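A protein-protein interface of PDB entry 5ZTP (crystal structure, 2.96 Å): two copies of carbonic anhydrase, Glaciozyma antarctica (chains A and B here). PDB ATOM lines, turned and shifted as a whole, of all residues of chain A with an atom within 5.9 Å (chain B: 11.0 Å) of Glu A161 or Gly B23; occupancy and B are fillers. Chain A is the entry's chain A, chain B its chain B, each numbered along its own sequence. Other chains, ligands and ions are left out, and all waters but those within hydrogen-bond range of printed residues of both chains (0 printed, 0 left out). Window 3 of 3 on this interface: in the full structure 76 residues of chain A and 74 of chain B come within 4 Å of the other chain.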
ATOM      1  N   THR A  91      27.763 -23.270   5.119  1.00  0.00           N
ATOM      2  CA  THR A  91      27.959 -22.129   5.937  1.00  0.00           C
ATOM      3  C   THR A  91      29.245 -22.444   6.693  1.00  0.00           C
ATOM      4  O   THR A  91      29.390 -23.552   7.182  1.00  0.00           O
ATOM      5  CB  THR A  91      26.673 -22.085   6.806  1.00  0.00           C
ATOM      6  OG1 THR A  91      25.779 -21.088   6.294  1.00  0.00           O
ATOM      7  CG2 THR A  91      26.938 -21.867   8.257  1.00  0.00           C
ATOM      8  N   ASP A  92      30.173 -21.501   6.777  1.00  0.00           N
ATOM      9  CA  ASP A  92      31.520 -21.764   7.341  1.00  0.00           C
ATOM     10  C   ASP A  92      32.354 -22.571   6.335  1.00  0.00           C
ATOM     11  O   ASP A  92      33.171 -23.430   6.719  1.00  0.00           O
ATOM     12  CB  ASP A  92      31.468 -22.484   8.728  1.00  0.00           C
ATOM     13  CG  ASP A  92      32.815 -22.444   9.493  1.00  0.00           C
ATOM     14  OD1 ASP A  92      33.490 -21.413   9.454  1.00  0.00           O
ATOM     15  OD2 ASP A  92      33.198 -23.441  10.152  1.00  0.00           O
ATOM     16  N   TYR A 158      23.390 -25.651   3.148  1.00  0.00           N
ATOM     17  CA  TYR A 158      23.519 -26.446   4.351  1.00  0.00           C
ATOM     18  C   TYR A 158      24.055 -25.586   5.492  1.00  0.00           C
ATOM     19  O   TYR A 158      25.107 -24.975   5.342  1.00  0.00           O
ATOM     20  CB  TYR A 158      24.455 -27.633   4.139  1.00  0.00           C
ATOM     21  CG  TYR A 158      24.593 -28.492   5.372  1.00  0.00           C
ATOM     22  CD1 TYR A 158      23.574 -29.349   5.776  1.00  0.00           C
ATOM     23  CD2 TYR A 158      25.727 -28.431   6.142  1.00  0.00           C
ATOM     24  CE1 TYR A 158      23.691 -30.120   6.909  1.00  0.00           C
ATOM     25  CE2 TYR A 158      25.848 -29.200   7.275  1.00  0.00           C
ATOM     26  CZ  TYR A 158      24.828 -30.038   7.649  1.00  0.00           C
ATOM     27  OH  TYR A 158      25.004 -30.786   8.789  1.00  0.00           O
ATOM     28  N   GLU A 159      23.335 -25.534   6.617  1.00  0.00           N
ATOM     29  CA  GLU A 159      23.831 -24.872   7.818  1.00  0.00           C
ATOM     30  C   GLU A 159      24.525 -25.835   8.765  1.00  0.00           C
ATOM     31  O   GLU A 159      23.897 -26.691   9.339  1.00  0.00           O
ATOM     32  CB  GLU A 159      22.693 -24.199   8.541  1.00  0.00           C
ATOM     33  CG  GLU A 159      22.467 -22.769   8.102  1.00  0.00           C
ATOM     34  CD  GLU A 159      21.031 -22.355   8.290  1.00  0.00           C
ATOM     35  OE1 GLU A 159      20.403 -22.847   9.282  1.00  0.00           O
ATOM     36  OE2 GLU A 159      20.541 -21.561   7.432  1.00  0.00           O
ATOM     37  N   VAL A 160      25.833 -25.667   8.938  1.00  0.00           N
ATOM     38  CA  VAL A 160      26.650 -26.560   9.775  1.00  0.00           C
ATOM     39  C   VAL A 160      26.310 -26.439  11.248  1.00  0.00           C
ATOM     40  O   VAL A 160      26.673 -27.305  12.041  1.00  0.00           O
ATOM     41  CB  VAL A 160      28.170 -26.287   9.620  1.00  0.00           C
ATOM     42  CG1 VAL A 160      28.625 -26.558   8.191  1.00  0.00           C
ATOM     43  CG2 VAL A 160      28.524 -24.872  10.068  1.00  0.00           C
ATOM     44  N   GLU A 161      25.634 -25.346  11.596  1.00  0.00           N
ATOM     45  CA  GLU A 161      25.177 -25.083  12.961  1.00  0.00           C
ATOM     46  C   GLU A 161      23.894 -25.871  13.264  1.00  0.00           C
ATOM     47  O   GLU A 161      23.837 -26.598  14.237  1.00  0.00           O
ATOM     48  CB  GLU A 161      24.937 -23.573  13.188  1.00  0.00           C
ATOM     49  CG  GLU A 161      26.130 -22.663  12.894  1.00  0.00           C
ATOM     50  CD  GLU A 161      26.238 -22.247  11.418  1.00  0.00           C
ATOM     51  OE1 GLU A 161      25.404 -22.686  10.578  1.00  0.00           O
ATOM     52  OE2 GLU A 161      27.168 -21.466  11.088  1.00  0.00           O
ATOM     53  N   THR A 162      22.878 -25.743  12.420  1.00  0.00           N
ATOM     54  CA  THR A 162      21.605 -26.417  12.646  1.00  0.00           C
ATOM     55  C   THR A 162      21.502 -27.793  12.009  1.00  0.00           C
ATOM     56  O   THR A 162      20.797 -28.659  12.518  1.00  0.00           O
ATOM     57  CB  THR A 162      20.450 -25.554  12.132  1.00  0.00           C
ATOM     58  OG1 THR A 162      20.704 -25.150  10.783  1.00  0.00           O
ATOM     59  CG2 THR A 162      20.318 -24.314  12.994  1.00  0.00           C
ATOM     60  N   GLY A 163      22.212 -28.000  10.907  1.00  0.00           N
ATOM     61  CA  GLY A 163      22.056 -29.207  10.071  1.00  0.00           C
ATOM     62  C   GLY A 163      20.934 -29.060   9.037  1.00  0.00           C
ATOM     63  O   GLY A 163      20.524 -30.036   8.418  1.00  0.00           O
ATOM     64  N   ASN B  12      15.208 -33.979   5.879  1.00  0.00           N
ATOM     65  CA  ASN B  12      16.128 -33.103   6.576  1.00  0.00           C
ATOM     66  C   ASN B  12      15.583 -32.775   7.959  1.00  0.00           C
ATOM     67  O   ASN B  12      16.325 -32.814   8.928  1.00  0.00           O
ATOM     68  CB  ASN B  12      16.406 -31.826   5.754  1.00  0.00           C
ATOM     69  CG  ASN B  12      17.546 -30.978   6.331  1.00  0.00           C
ATOM     70  OD1 ASN B  12      17.344 -29.817   6.700  1.00  0.00           O
ATOM     71  ND2 ASN B  12      18.742 -31.560   6.423  1.00  0.00           N
ATOM     72  N   TYR B  15      16.794 -35.366   9.974  1.00  0.00           N
ATOM     73  CA  TYR B  15      18.239 -35.274  10.187  1.00  0.00           C
ATOM     74  C   TYR B  15      18.572 -34.202  11.216  1.00  0.00           C
ATOM     75  O   TYR B  15      19.499 -34.363  12.006  1.00  0.00           O
ATOM     76  CB  TYR B  15      18.950 -34.942   8.870  1.00  0.00           C
ATOM     77  CG  TYR B  15      20.461 -34.846   8.985  1.00  0.00           C
ATOM     78  CD1 TYR B  15      21.250 -35.995   9.122  1.00  0.00           C
ATOM     79  CD2 TYR B  15      21.107 -33.593   8.955  1.00  0.00           C
ATOM     80  CE1 TYR B  15      22.627 -35.908   9.229  1.00  0.00           C
ATOM     81  CE2 TYR B  15      22.492 -33.491   9.072  1.00  0.00           C
ATOM     82  CZ  TYR B  15      23.244 -34.645   9.199  1.00  0.00           C
ATOM     83  OH  TYR B  15      24.610 -34.537   9.304  1.00  0.00           O
ATOM     84  N   VAL B  16      17.806 -33.108  11.166  1.00  0.00           N
ATOM     85  CA  VAL B  16      17.910 -32.001  12.103  1.00  0.00           C
ATOM     86  C   VAL B  16      17.423 -32.422  13.483  1.00  0.00           C
ATOM     87  O   VAL B  16      18.087 -32.129  14.476  1.00  0.00           O
ATOM     88  CB  VAL B  16      17.073 -30.789  11.667  1.00  0.00           C
ATOM     89  CG1 VAL B  16      17.055 -29.761  12.763  1.00  0.00           C
ATOM     90  CG2 VAL B  16      17.626 -30.169  10.402  1.00  0.00           C
ATOM     91  N   ALA B  17      16.259 -33.084  13.549  1.00  0.00           N
ATOM     92  CA  ALA B  17      15.741 -33.595  14.821  1.00  0.00           C
ATOM     93  C   ALA B  17      16.765 -34.562  15.457  1.00  0.00           C
ATOM     94  O   ALA B  17      16.970 -34.535  16.656  1.00  0.00           O
ATOM     95  CB  ALA B  17      14.398 -34.262  14.626  1.00  0.00           C
ATOM     96  N   ALA B  18      17.449 -35.375  14.650  1.00  0.00           N
ATOM     97  CA  ALA B  18      18.547 -36.251  15.137  1.00  0.00           C
ATOM     98  C   ALA B  18      19.912 -35.541  15.305  1.00  0.00           C
ATOM     99  O   ALA B  18      20.880 -36.157  15.768  1.00  0.00           O
ATOM    100  CB  ALA B  18      18.711 -37.447  14.203  1.00  0.00           C
ATOM    101  N   PHE B  19      19.983 -34.257  14.959  1.00  0.00           N
ATOM    102  CA  PHE B  19      21.256 -33.537  14.890  1.00  0.00           C
ATOM    103  C   PHE B  19      21.659 -33.299  16.334  1.00  0.00           C
ATOM    104  O   PHE B  19      21.049 -32.466  17.005  1.00  0.00           O
ATOM    105  CB  PHE B  19      21.062 -32.190  14.211  1.00  0.00           C
ATOM    106  CG  PHE B  19      22.297 -31.625  13.586  1.00  0.00           C
ATOM    107  CD1 PHE B  19      22.999 -32.344  12.629  1.00  0.00           C
ATOM    108  CD2 PHE B  19      22.718 -30.347  13.894  1.00  0.00           C
ATOM    109  CE1 PHE B  19      24.128 -31.819  12.031  1.00  0.00           C
ATOM    110  CE2 PHE B  19      23.838 -29.818  13.301  1.00  0.00           C
ATOM    111  CZ  PHE B  19      24.551 -30.555  12.371  1.00  0.00           C
ATOM    112  N   GLY B  20      22.616 -34.037  16.868  1.00  0.00           N
ATOM    113  CA  GLY B  20      22.810 -33.983  18.316  1.00  0.00           C
ATOM    114  C   GLY B  20      23.691 -32.799  18.632  1.00  0.00           C
ATOM    115  O   GLY B  20      23.282 -31.647  18.506  1.00  0.00           O
ATOM    116  N   ASP B  21      24.932 -33.106  18.977  1.00  0.00           N
ATOM    117  CA  ASP B  21      25.936 -32.087  19.205  1.00  0.00           C
ATOM    118  C   ASP B  21      26.717 -31.694  17.976  1.00  0.00           C
ATOM    119  O   ASP B  21      27.647 -30.911  18.065  1.00  0.00           O
ATOM    120  CB  ASP B  21      26.882 -32.546  20.296  1.00  0.00           C
ATOM    121  CG  ASP B  21      26.391 -32.147  21.654  1.00  0.00           C
ATOM    122  OD1 ASP B  21      25.383 -31.401  21.732  1.00  0.00           O
ATOM    123  OD2 ASP B  21      27.003 -32.574  22.648  1.00  0.00           O
ATOM    124  N   LYS B  22      26.312 -32.185  16.818  1.00  0.00           N
ATOM    125  CA  LYS B  22      27.051 -31.926  15.592  1.00  0.00           C
ATOM    126  C   LYS B  22      27.049 -30.454  15.211  1.00  0.00           C
ATOM    127  O   LYS B  22      27.869 -30.010  14.401  1.00  0.00           O
ATOM    128  CB  LYS B  22      26.521 -32.788  14.437  1.00  0.00           C
ATOM    129  CG  LYS B  22      27.080 -34.212  14.446  1.00  0.00           C
ATOM    130  CD  LYS B  22      26.168 -35.177  13.716  1.00  0.00           C
ATOM    131  CE  LYS B  22      25.040 -35.638  14.624  1.00  0.00           C
ATOM    132  NZ  LYS B  22      23.793 -35.985  13.881  1.00  0.00           N
ATOM    133  N   GLY B  23      26.162 -29.683  15.825  1.00  0.00           N
ATOM    134  CA  GLY B  23      26.098 -28.263  15.526  1.00  0.00           C
ATOM    135  C   GLY B  23      27.398 -27.481  15.595  1.00  0.00           C
ATOM    136  O   GLY B  23      27.503 -26.419  14.995  1.00  0.00           O
ATOM    137  N   SER B  24      28.379 -27.997  16.319  1.00  0.00           N
ATOM    138  CA  SER B  24      29.515 -27.203  16.748  1.00  0.00           C
ATOM    139  C   SER B  24      30.826 -27.864  16.334  1.00  0.00           C
ATOM    140  O   SER B  24      31.880 -27.676  16.940  1.00  0.00           O
ATOM    141  CB  SER B  24      29.463 -27.065  18.269  1.00  0.00           C
ATOM    142  OG  SER B  24      29.748 -28.321  18.869  1.00  0.00           O
ATOM    143  N   LEU B  25      30.754 -28.683  15.312  1.00  0.00           N
ATOM    144  CA  LEU B  25      31.944 -29.231  14.753  1.00  0.00           C
ATOM    145  C   LEU B  25      32.546 -28.126  13.887  1.00  0.00           C
ATOM    146  O   LEU B  25      31.845 -27.486  13.105  1.00  0.00           O
ATOM    147  CB  LEU B  25      31.580 -30.408  13.872  1.00  0.00           C
ATOM    148  CG  LEU B  25      31.129 -31.700  14.529  1.00  0.00           C
ATOM    149  CD1 LEU B  25      30.322 -32.500  13.518  1.00  0.00           C
ATOM    150  CD2 LEU B  25      32.361 -32.463  14.950  1.00  0.00           C
ATOM    151  N   PRO B  26      33.843 -27.909  13.996  1.00  0.00           N
ATOM    152  CA  PRO B  26      34.448 -26.872  13.207  1.00  0.00           C
ATOM    153  C   PRO B  26      34.944 -27.343  11.841  1.00  0.00           C
ATOM    154  O   PRO B  26      34.825 -28.519  11.477  1.00  0.00           O
ATOM    155  CB  PRO B  26      35.626 -26.465  14.075  1.00  0.00           C
ATOM    156  CG  PRO B  26      36.074 -27.777  14.654  1.00  0.00           C
ATOM    157  CD  PRO B  26      34.817 -28.586  14.863  1.00  0.00           C
ATOM    158  N   LEU B  27      35.569 -26.413  11.125  1.00  0.00           N
ATOM    159  CA  LEU B  27      36.001 -26.601   9.739  1.00  0.00           C
ATOM    160  C   LEU B  27      37.068 -27.682   9.442  1.00  0.00           C
ATOM    161  O   LEU B  27      36.811 -28.546   8.614  1.00  0.00           O
ATOM    162  CB  LEU B  27      36.440 -25.237   9.184  1.00  0.00           C
ATOM    163  CG  LEU B  27      36.617 -25.036   7.679  1.00  0.00           C
ATOM    164  CD1 LEU B  27      35.589 -25.812   6.844  1.00  0.00           C
ATOM    165  CD2 LEU B  27      36.552 -23.546   7.356  1.00  0.00           C
ATOM    166  N   GLU B  53      30.292 -37.157  10.782  1.00  0.00           N
ATOM    167  CA  GLU B  53      30.361 -35.735  10.583  1.00  0.00           C
ATOM    168  C   GLU B  53      31.596 -35.126  11.230  1.00  0.00           C
ATOM    169  O   GLU B  53      31.828 -35.314  12.420  1.00  0.00           O
ATOM    170  CB  GLU B  53      29.090 -35.061  11.112  1.00  0.00           C
ATOM    171  CG  GLU B  53      27.868 -35.196  10.200  1.00  0.00           C
ATOM    172  CD  GLU B  53      27.088 -36.485  10.401  1.00  0.00           C
ATOM    173  OE1 GLU B  53      27.661 -37.437  10.980  1.00  0.00           O
ATOM    174  OE2 GLU B  53      25.902 -36.530   9.977  1.00  0.00           O
ATOM    175  N   GLY B  54      32.390 -34.422  10.417  1.00  0.00           N
ATOM    176  CA  GLY B  54      33.565 -33.677  10.873  1.00  0.00           C
ATOM    177  C   GLY B  54      34.883 -34.425  10.739  1.00  0.00           C
ATOM    178  O   GLY B  54      35.944 -33.837  10.898  1.00  0.00           O
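No position is printed for both chains. Of the 14 pairs that touch across the chains among the printed residues, none has its exchanged pair printed and touching as well.
ND2 of Asn B12 is in hydrogen-bond range of O of Gly A163 (3.1 Å). The backbone carbonyl oxygen of Val A160 lies close to the backbone carbonyl oxygen of Gly B23.
Hydrophobic or aromatic side chains of chain A that line the printed part of chain B: Tyr A158. Printed residues of chain B that touch a printed residue of chain A: Asn B12, Tyr B15, Val B16, Phe B19, Lys B22, Gly B23 and Leu B27. Hydrophobic or aromatic side chains of chain B that line the printed part of chain A: Tyr B15, Val B16, Phe B19 and Leu B27. Among the printed residues, no Asp or Glu carboxylate lies within 4 Å of a Lys or Arg side-chain nitrogen of the other chain.
Among the printed residues, merely in contact across the chains: Asp A92 with Leu B27, Tyr A158 with Tyr B15, Tyr A158 with Phe B19, Val A160 with Phe B19, Val A160 with Lys B22, Glu A161 with Phe B19, Glu A161 with Gly B23, Thr A162 with Val B16, Thr A162 with Phe B19, Gly A163 with Tyr B15, Gly A163 with Val B16 and Gly A163 with Phe B19.
N of Thr A91 is in hydrogen-bond range of O of Tyr A158 (3.2 Å). The side-chain carboxylate of Glu A159 lies within hydrogen-bond range of the side-chain hydroxyl of Thr A162 (2.8 Å). OH of Tyr B15 is in hydrogen-bond range of OE2 of Glu B53. NZ of Lys B22 lies within hydrogen-bond range of O of Ala B18 (3.5 Å).
No residue of chain B comes within 4 Å of Thr A91. No residue of chain B comes within 4 Å of Glu A159. Of chain B, only Phe B19 (3.9 Å), Lys B22 (3.8 Å) and Gly B23 (3.2 Å) come within 4 Å of Val A160. Of chain B, only Phe B19 (3.4 Å) and Gly B23 (3.1 Å) come within 4 Å of Glu A161. Thr A162 touches two residues of chain B. Of the printed residues of chain B, Gly A163 touches Asn B12, Tyr B15, Val B16 and Phe B19. Printed residues of chain A within 4 Å of Phe B19: Tyr A158, Val A160, Glu A161, Thr A162 and Gly A163. Printed residues of chain A within 4 Å of Leu B27: Asp A92.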
